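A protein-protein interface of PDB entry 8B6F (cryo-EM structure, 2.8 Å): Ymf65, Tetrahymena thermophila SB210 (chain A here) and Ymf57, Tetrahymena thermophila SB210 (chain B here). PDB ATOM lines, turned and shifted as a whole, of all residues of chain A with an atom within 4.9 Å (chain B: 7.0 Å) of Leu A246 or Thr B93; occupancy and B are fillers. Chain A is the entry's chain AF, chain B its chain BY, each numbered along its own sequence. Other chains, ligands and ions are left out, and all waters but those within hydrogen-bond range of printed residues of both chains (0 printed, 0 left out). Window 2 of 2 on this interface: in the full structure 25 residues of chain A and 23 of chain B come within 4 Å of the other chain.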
ATOM      1  N   ASN A 242     -32.819  19.557  -4.002  1.00  0.00           N
ATOM      2  CA  ASN A 242     -31.654  20.303  -4.462  1.00  0.00           C
ATOM      3  C   ASN A 242     -31.878  20.879  -5.851  1.00  0.00           C
ATOM      4  O   ASN A 242     -31.364  21.957  -6.166  1.00  0.00           O
ATOM      5  CB  ASN A 242     -30.420  19.403  -4.454  1.00  0.00           C
ATOM      6  CG  ASN A 242     -30.109  18.854  -3.077  1.00  0.00           C
ATOM      7  OD1 ASN A 242     -30.394  19.490  -2.063  1.00  0.00           O
ATOM      8  ND2 ASN A 242     -29.522  17.666  -3.034  1.00  0.00           N
ATOM      9  N   ILE A 243     -32.627  20.174  -6.699  1.00  0.00           N
ATOM     10  CA  ILE A 243     -32.915  20.688  -8.033  1.00  0.00           C
ATOM     11  C   ILE A 243     -33.671  22.008  -7.937  1.00  0.00           C
ATOM     12  O   ILE A 243     -33.323  22.992  -8.597  1.00  0.00           O
ATOM     13  CB  ILE A 243     -33.706  19.648  -8.847  1.00  0.00           C
ATOM     14  CG1 ILE A 243     -32.908  18.346  -8.964  1.00  0.00           C
ATOM     15  CG2 ILE A 243     -34.034  20.196 -10.233  1.00  0.00           C
ATOM     16  CD1 ILE A 243     -33.657  17.220  -9.650  1.00  0.00           C
ATOM     17  N   THR A 244     -34.723  22.046  -7.114  1.00  0.00           N
ATOM     18  CA  THR A 244     -35.512  23.269  -6.992  1.00  0.00           C
ATOM     19  C   THR A 244     -34.696  24.404  -6.384  1.00  0.00           C
ATOM     20  O   THR A 244     -34.751  25.540  -6.866  1.00  0.00           O
ATOM     21  CB  THR A 244     -36.760  23.003  -6.151  1.00  0.00           C
ATOM     22  OG1 THR A 244     -37.542  21.971  -6.763  1.00  0.00           O
ATOM     23  CG2 THR A 244     -37.605  24.265  -6.018  1.00  0.00           C
ATOM     24  N   LEU A 245     -33.932  24.119  -5.327  1.00  0.00           N
ATOM     25  CA  LEU A 245     -33.128  25.164  -4.704  1.00  0.00           C
ATOM     26  C   LEU A 245     -32.097  25.703  -5.684  1.00  0.00           C
ATOM     27  O   LEU A 245     -31.905  26.918  -5.800  1.00  0.00           O
ATOM     28  CB  LEU A 245     -32.448  24.629  -3.444  1.00  0.00           C
ATOM     29  CG  LEU A 245     -33.380  24.272  -2.284  1.00  0.00           C
ATOM     30  CD1 LEU A 245     -32.610  23.562  -1.188  1.00  0.00           C
ATOM     31  CD2 LEU A 245     -34.063  25.513  -1.736  1.00  0.00           C
ATOM     32  N   LEU A 246     -31.415  24.806  -6.393  1.00  0.00           N
ATOM     33  CA  LEU A 246     -30.423  25.236  -7.369  1.00  0.00           C
ATOM     34  C   LEU A 246     -31.061  26.053  -8.484  1.00  0.00           C
ATOM     35  O   LEU A 246     -30.484  27.043  -8.947  1.00  0.00           O
ATOM     36  CB  LEU A 246     -29.704  24.016  -7.943  1.00  0.00           C
ATOM     37  CG  LEU A 246     -28.785  24.259  -9.139  1.00  0.00           C
ATOM     38  CD1 LEU A 246     -27.668  25.224  -8.780  1.00  0.00           C
ATOM     39  CD2 LEU A 246     -28.231  22.935  -9.629  1.00  0.00           C
ATOM     40  N   PHE A 247     -32.253  25.655  -8.930  1.00  0.00           N
ATOM     41  CA  PHE A 247     -32.908  26.380 -10.014  1.00  0.00           C
ATOM     42  C   PHE A 247     -33.370  27.760  -9.565  1.00  0.00           C
ATOM     43  O   PHE A 247     -33.299  28.723 -10.337  1.00  0.00           O
ATOM     44  CB  PHE A 247     -34.084  25.577 -10.559  1.00  0.00           C
ATOM     45  CG  PHE A 247     -34.574  26.078 -11.881  1.00  0.00           C
ATOM     46  CD1 PHE A 247     -33.897  25.753 -13.044  1.00  0.00           C
ATOM     47  CD2 PHE A 247     -35.688  26.894 -11.963  1.00  0.00           C
ATOM     48  CE1 PHE A 247     -34.330  26.214 -14.267  1.00  0.00           C
ATOM     49  CE2 PHE A 247     -36.126  27.361 -13.187  1.00  0.00           C
ATOM     50  CZ  PHE A 247     -35.444  27.020 -14.340  1.00  0.00           C
ATOM     51  N   ILE A 248     -33.852  27.882  -8.327  1.00  0.00           N
ATOM     52  CA  ILE A 248     -34.220  29.197  -7.809  1.00  0.00           C
ATOM     53  C   ILE A 248     -32.997  30.103  -7.773  1.00  0.00           C
ATOM     54  O   ILE A 248     -33.042  31.260  -8.203  1.00  0.00           O
ATOM     55  CB  ILE A 248     -34.867  29.061  -6.418  1.00  0.00           C
ATOM     56  CG1 ILE A 248     -36.235  28.385  -6.539  1.00  0.00           C
ATOM     57  CG2 ILE A 248     -35.001  30.422  -5.739  1.00  0.00           C
ATOM     58  CD1 ILE A 248     -36.851  27.991  -5.212  1.00  0.00           C
ATOM     59  N   CYS A 249     -31.885  29.587  -7.254  1.00  0.00           N
ATOM     60  CA  CYS A 249     -30.659  30.372  -7.199  1.00  0.00           C
ATOM     61  C   CYS A 249     -30.201  30.766  -8.597  1.00  0.00           C
ATOM     62  O   CYS A 249     -29.793  31.910  -8.828  1.00  0.00           O
ATOM     63  CB  CYS A 249     -29.579  29.585  -6.465  1.00  0.00           C
ATOM     64  SG  CYS A 249     -29.988  29.343  -4.729  1.00  0.00           S
ATOM     65  N   LEU A 250     -30.252  29.828  -9.541  1.00  0.00           N
ATOM     66  CA  LEU A 250     -29.834  30.123 -10.905  1.00  0.00           C
ATOM     67  C   LEU A 250     -30.718  31.186 -11.535  1.00  0.00           C
ATOM     68  O   LEU A 250     -30.225  32.103 -12.199  1.00  0.00           O
ATOM     69  CB  LEU A 250     -29.883  28.851 -11.741  1.00  0.00           C
ATOM     70  CG  LEU A 250     -28.767  27.864 -11.446  1.00  0.00           C
ATOM     71  CD1 LEU A 250     -29.170  26.514 -11.969  1.00  0.00           C
ATOM     72  CD2 LEU A 250     -27.475  28.338 -12.090  1.00  0.00           C
ATOM     73  N   PHE A 310     -25.314  27.148  -2.382  1.00  0.00           N
ATOM     74  CA  PHE A 310     -25.555  27.034  -3.815  1.00  0.00           C
ATOM     75  C   PHE A 310     -24.956  28.181  -4.614  1.00  0.00           C
ATOM     76  O   PHE A 310     -24.526  27.970  -5.751  1.00  0.00           O
ATOM     77  CB  PHE A 310     -27.060  26.979  -4.098  1.00  0.00           C
ATOM     78  CG  PHE A 310     -27.741  25.747  -3.574  1.00  0.00           C
ATOM     79  CD1 PHE A 310     -27.762  24.581  -4.317  1.00  0.00           C
ATOM     80  CD2 PHE A 310     -28.386  25.766  -2.348  1.00  0.00           C
ATOM     81  CE1 PHE A 310     -28.398  23.449  -3.840  1.00  0.00           C
ATOM     82  CE2 PHE A 310     -29.023  24.638  -1.866  1.00  0.00           C
ATOM     83  CZ  PHE A 310     -29.029  23.479  -2.613  1.00  0.00           C
ATOM     84  N   ILE A 314     -22.180  28.784  -8.591  1.00  0.00           N
ATOM     85  CA  ILE A 314     -22.702  29.580  -9.699  1.00  0.00           C
ATOM     86  C   ILE A 314     -21.846  30.822  -9.900  1.00  0.00           C
ATOM     87  O   ILE A 314     -21.496  31.178 -11.031  1.00  0.00           O
ATOM     88  CB  ILE A 314     -24.178  29.943  -9.453  1.00  0.00           C
ATOM     89  CG1 ILE A 314     -25.013  28.677  -9.247  1.00  0.00           C
ATOM     90  CG2 ILE A 314     -24.728  30.744 -10.624  1.00  0.00           C
ATOM     91  CD1 ILE A 314     -26.428  28.943  -8.780  1.00  0.00           C
ATOM     92  N   ILE A 317     -18.459  29.802 -11.493  1.00  0.00           N
ATOM     93  CA  ILE A 317     -18.577  29.471 -12.911  1.00  0.00           C
ATOM     94  C   ILE A 317     -18.768  30.740 -13.732  1.00  0.00           C
ATOM     95  O   ILE A 317     -18.132  30.930 -14.773  1.00  0.00           O
ATOM     96  CB  ILE A 317     -19.725  28.471 -13.137  1.00  0.00           C
ATOM     97  CG1 ILE A 317     -19.408  27.140 -12.449  1.00  0.00           C
ATOM     98  CG2 ILE A 317     -19.961  28.249 -14.627  1.00  0.00           C
ATOM     99  CD1 ILE A 317     -20.565  26.169 -12.416  1.00  0.00           C
ATOM    100  N   LEU B  87     -30.002  28.149 -20.319  1.00  0.00           N
ATOM    101  CA  LEU B  87     -30.135  26.699 -20.413  1.00  0.00           C
ATOM    102  C   LEU B  87     -28.885  25.983 -19.923  1.00  0.00           C
ATOM    103  O   LEU B  87     -28.974  25.016 -19.157  1.00  0.00           O
ATOM    104  CB  LEU B  87     -30.452  26.295 -21.854  1.00  0.00           C
ATOM    105  CG  LEU B  87     -31.844  26.660 -22.375  1.00  0.00           C
ATOM    106  CD1 LEU B  87     -31.960  26.327 -23.851  1.00  0.00           C
ATOM    107  CD2 LEU B  87     -32.932  25.948 -21.587  1.00  0.00           C
ATOM    108  N   TYR B  88     -27.709  26.428 -20.360  1.00  0.00           N
ATOM    109  CA  TYR B  88     -26.508  25.631 -20.153  1.00  0.00           C
ATOM    110  C   TYR B  88     -25.813  25.897 -18.828  1.00  0.00           C
ATOM    111  O   TYR B  88     -25.080  25.025 -18.351  1.00  0.00           O
ATOM    112  CB  TYR B  88     -25.535  25.840 -21.314  1.00  0.00           C
ATOM    113  CG  TYR B  88     -26.026  25.153 -22.562  1.00  0.00           C
ATOM    114  CD1 TYR B  88     -25.848  23.788 -22.736  1.00  0.00           C
ATOM    115  CD2 TYR B  88     -26.706  25.856 -23.546  1.00  0.00           C
ATOM    116  CE1 TYR B  88     -26.312  23.145 -23.860  1.00  0.00           C
ATOM    117  CE2 TYR B  88     -27.175  25.222 -24.676  1.00  0.00           C
ATOM    118  CZ  TYR B  88     -26.973  23.866 -24.829  1.00  0.00           C
ATOM    119  OH  TYR B  88     -27.437  23.229 -25.953  1.00  0.00           O
ATOM    120  N   LEU B  89     -26.010  27.066 -18.216  1.00  0.00           N
ATOM    121  CA  LEU B  89     -25.588  27.210 -16.829  1.00  0.00           C
ATOM    122  C   LEU B  89     -26.363  26.249 -15.944  1.00  0.00           C
ATOM    123  O   LEU B  89     -25.798  25.625 -15.040  1.00  0.00           O
ATOM    124  CB  LEU B  89     -25.771  28.650 -16.350  1.00  0.00           C
ATOM    125  CG  LEU B  89     -25.047  28.962 -15.035  1.00  0.00           C
ATOM    126  CD1 LEU B  89     -23.536  28.937 -15.209  1.00  0.00           C
ATOM    127  CD2 LEU B  89     -25.472  30.290 -14.488  1.00  0.00           C
ATOM    128  N   PHE B  90     -27.670  26.131 -16.182  1.00  0.00           N
ATOM    129  CA  PHE B  90     -28.462  25.141 -15.466  1.00  0.00           C
ATOM    130  C   PHE B  90     -27.968  23.728 -15.749  1.00  0.00           C
ATOM    131  O   PHE B  90     -27.856  22.905 -14.833  1.00  0.00           O
ATOM    132  CB  PHE B  90     -29.935  25.277 -15.848  1.00  0.00           C
ATOM    133  CG  PHE B  90     -30.770  24.098 -15.453  1.00  0.00           C
ATOM    134  CD1 PHE B  90     -31.111  23.888 -14.128  1.00  0.00           C
ATOM    135  CD2 PHE B  90     -31.217  23.199 -16.407  1.00  0.00           C
ATOM    136  CE1 PHE B  90     -31.879  22.802 -13.761  1.00  0.00           C
ATOM    137  CE2 PHE B  90     -31.984  22.112 -16.047  1.00  0.00           C
ATOM    138  CZ  PHE B  90     -32.318  21.914 -14.723  1.00  0.00           C
ATOM    139  N   PHE B  91     -27.667  23.428 -17.014  1.00  0.00           N
ATOM    140  CA  PHE B  91     -27.192  22.095 -17.364  1.00  0.00           C
ATOM    141  C   PHE B  91     -25.887  21.761 -16.652  1.00  0.00           C
ATOM    142  O   PHE B  91     -25.725  20.661 -16.115  1.00  0.00           O
ATOM    143  CB  PHE B  91     -27.008  21.971 -18.875  1.00  0.00           C
ATOM    144  CG  PHE B  91     -26.252  20.741 -19.279  1.00  0.00           C
ATOM    145  CD1 PHE B  91     -26.901  19.525 -19.391  1.00  0.00           C
ATOM    146  CD2 PHE B  91     -24.889  20.793 -19.522  1.00  0.00           C
ATOM    147  CE1 PHE B  91     -26.213  18.387 -19.748  1.00  0.00           C
ATOM    148  CE2 PHE B  91     -24.195  19.657 -19.880  1.00  0.00           C
ATOM    149  CZ  PHE B  91     -24.858  18.452 -19.994  1.00  0.00           C
ATOM    150  N   ILE B  92     -24.932  22.692 -16.650  1.00  0.00           N
ATOM    151  CA  ILE B  92     -23.638  22.392 -16.048  1.00  0.00           C
ATOM    152  C   ILE B  92     -23.763  22.266 -14.538  1.00  0.00           C
ATOM    153  O   ILE B  92     -23.104  21.426 -13.914  1.00  0.00           O
ATOM    154  CB  ILE B  92     -22.603  23.460 -16.452  1.00  0.00           C
ATOM    155  CG1 ILE B  92     -21.186  22.889 -16.373  1.00  0.00           C
ATOM    156  CG2 ILE B  92     -22.710  24.711 -15.582  1.00  0.00           C
ATOM    157  CD1 ILE B  92     -20.866  21.882 -17.454  1.00  0.00           C
ATOM    158  N   THR B  93     -24.598  23.099 -13.922  1.00  0.00           N
ATOM    159  CA  THR B  93     -24.806  22.994 -12.484  1.00  0.00           C
ATOM    160  C   THR B  93     -25.477  21.679 -12.114  1.00  0.00           C
ATOM    161  O   THR B  93     -25.112  21.050 -11.115  1.00  0.00           O
ATOM    162  CB  THR B  93     -25.626  24.182 -12.005  1.00  0.00           C
ATOM    163  OG1 THR B  93     -26.761  24.332 -12.865  1.00  0.00           O
ATOM    164  CG2 THR B  93     -24.792  25.449 -12.023  1.00  0.00           C
ATOM    165  N   ILE B  94     -26.466  21.245 -12.901  1.00  0.00           N
ATOM    166  CA  ILE B  94     -27.119  19.974 -12.609  1.00  0.00           C
ATOM    167  C   ILE B  94     -26.156  18.824 -12.858  1.00  0.00           C
ATOM    168  O   ILE B  94     -26.190  17.811 -12.151  1.00  0.00           O
ATOM    169  CB  ILE B  94     -28.420  19.830 -13.427  1.00  0.00           C
ATOM    170  CG1 ILE B  94     -29.492  19.105 -12.608  1.00  0.00           C
ATOM    171  CG2 ILE B  94     -28.196  19.064 -14.725  1.00  0.00           C
ATOM    172  CD1 ILE B  94     -30.048  19.910 -11.456  1.00  0.00           C
ATOM    173  N   PHE B  95     -25.288  18.953 -13.862  1.00  0.00           N
ATOM    174  CA  PHE B  95     -24.272  17.934 -14.091  1.00  0.00           C
ATOM    175  C   PHE B  95     -23.328  17.834 -12.901  1.00  0.00           C
ATOM    176  O   PHE B  95     -22.956  16.733 -12.483  1.00  0.00           O
ATOM    177  CB  PHE B  95     -23.502  18.253 -15.373  1.00  0.00           C
ATOM    178  CG  PHE B  95     -22.429  17.260 -15.698  1.00  0.00           C
ATOM    179  CD1 PHE B  95     -22.709  16.141 -16.462  1.00  0.00           C
ATOM    180  CD2 PHE B  95     -21.137  17.449 -15.239  1.00  0.00           C
ATOM    181  CE1 PHE B  95     -21.721  15.228 -16.761  1.00  0.00           C
ATOM    182  CE2 PHE B  95     -20.144  16.540 -15.535  1.00  0.00           C
ATOM    183  CZ  PHE B  95     -20.435  15.429 -16.297  1.00  0.00           C
ATOM    184  N   ILE B  96     -22.927  18.978 -12.344  1.00  0.00           N
ATOM    185  CA  ILE B  96     -22.107  18.964 -11.137  1.00  0.00           C
ATOM    186  C   ILE B  96     -22.881  18.340  -9.986  1.00  0.00           C
ATOM    187  O   ILE B  96     -22.332  17.567  -9.193  1.00  0.00           O
ATOM    188  CB  ILE B  96     -21.630  20.390 -10.801  1.00  0.00           C
ATOM    189  CG1 ILE B  96     -20.609  20.861 -11.841  1.00  0.00           C
ATOM    190  CG2 ILE B  96     -21.030  20.449  -9.398  1.00  0.00           C
ATOM    191  CD1 ILE B  96     -20.224  22.322 -11.717  1.00  0.00           C
ATOM    192  N   LEU B  97     -24.170  18.671  -9.871  1.00  0.00           N
ATOM    193  CA  LEU B  97     -24.970  18.154  -8.767  1.00  0.00           C
ATOM    194  C   LEU B  97     -25.075  16.635  -8.816  1.00  0.00           C
ATOM    195  O   LEU B  97     -24.951  15.965  -7.786  1.00  0.00           O
ATOM    196  CB  LEU B  97     -26.363  18.784  -8.800  1.00  0.00           C
ATOM    197  CG  LEU B  97     -27.346  18.356  -7.708  1.00  0.00           C
ATOM    198  CD1 LEU B  97     -26.845  18.774  -6.335  1.00  0.00           C
ATOM    199  CD2 LEU B  97     -28.718  18.943  -7.978  1.00  0.00           C
ATOM    200  N   PHE B  98     -25.301  16.074 -10.002  1.00  0.00           N
ATOM    201  CA  PHE B  98     -25.557  14.644 -10.128  1.00  0.00           C
ATOM    202  C   PHE B  98     -24.279  13.832 -10.299  1.00  0.00           C
ATOM    203  O   PHE B  98     -24.065  12.855  -9.575  1.00  0.00           O
ATOM    204  CB  PHE B  98     -26.490  14.376 -11.314  1.00  0.00           C
ATOM    205  CG  PHE B  98     -27.921  14.787 -11.084  1.00  0.00           C
ATOM    206  CD1 PHE B  98     -28.348  15.264  -9.853  1.00  0.00           C
ATOM    207  CD2 PHE B  98     -28.845  14.680 -12.108  1.00  0.00           C
ATOM    208  CE1 PHE B  98     -29.664  15.632  -9.658  1.00  0.00           C
ATOM    209  CE2 PHE B  98     -30.159  15.047 -11.918  1.00  0.00           C
ATOM    210  CZ  PHE B  98     -30.570  15.522 -10.693  1.00  0.00           C
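Among the printed residues, pairs that only touch across the chains: Asn A242 with Leu B97, Ile A243 with Phe B98, Leu A246 with Thr B93, Leu A246 with Ile B94, Phe A247 with Phe B90, Leu A250 with Leu B89, Leu A250 with Phe B90, Leu A250 with Thr B93, Ile A314 with Leu B89, Ile A317 with Leu B89 and Ile A317 with Ile B96.
The backbone carbonyl oxygen of Leu B89 sits at hydrogen-bond distance from the side-chain hydroxyl of Thr B93, at 2.7 Å.
The backbone carbonyl oxygen of Phe B90 sits at hydrogen-bond distance from the side-chain hydroxyl of Thr B93 (2.7 Å).
Of the 12 printed residues of chain B, 7 touch a printed residue of chain A.
Hydrophobic or aromatic side chains of chain A that line the printed part of chain B: Ile A243, Leu A246, Phe A247, Leu A250, Ile A314 and Ile A317.
Among the printed residues, 11 pairs touch across the chains.
Of the printed residues of chain B, Leu A246 touches Thr B93 and Ile B94.
Thr B93 touches two residues of chain A.
Printed residues of chain B within 4 Å of Leu A250: Leu B89, Phe B90 and Thr B93.
Printed residues of chain A within 4 Å of Phe B90: Phe A247 (3.5 Å) and Leu A250 (3.8 Å).
Of the printed residues of chain B, Ile A314 touches Leu B89.
Of the printed residues of chain A, Ile B94 touches Leu A246.
Of the printed residues of chain A, Phe B98 touches Ile A243 (3.7 Å).
The nearest residue of chain B that does not touch Leu A246 is Leu B97 (4.3 Å).
The nearest residue of chain A that does not touch Thr B93 is Ile A314 (4.3 Å).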
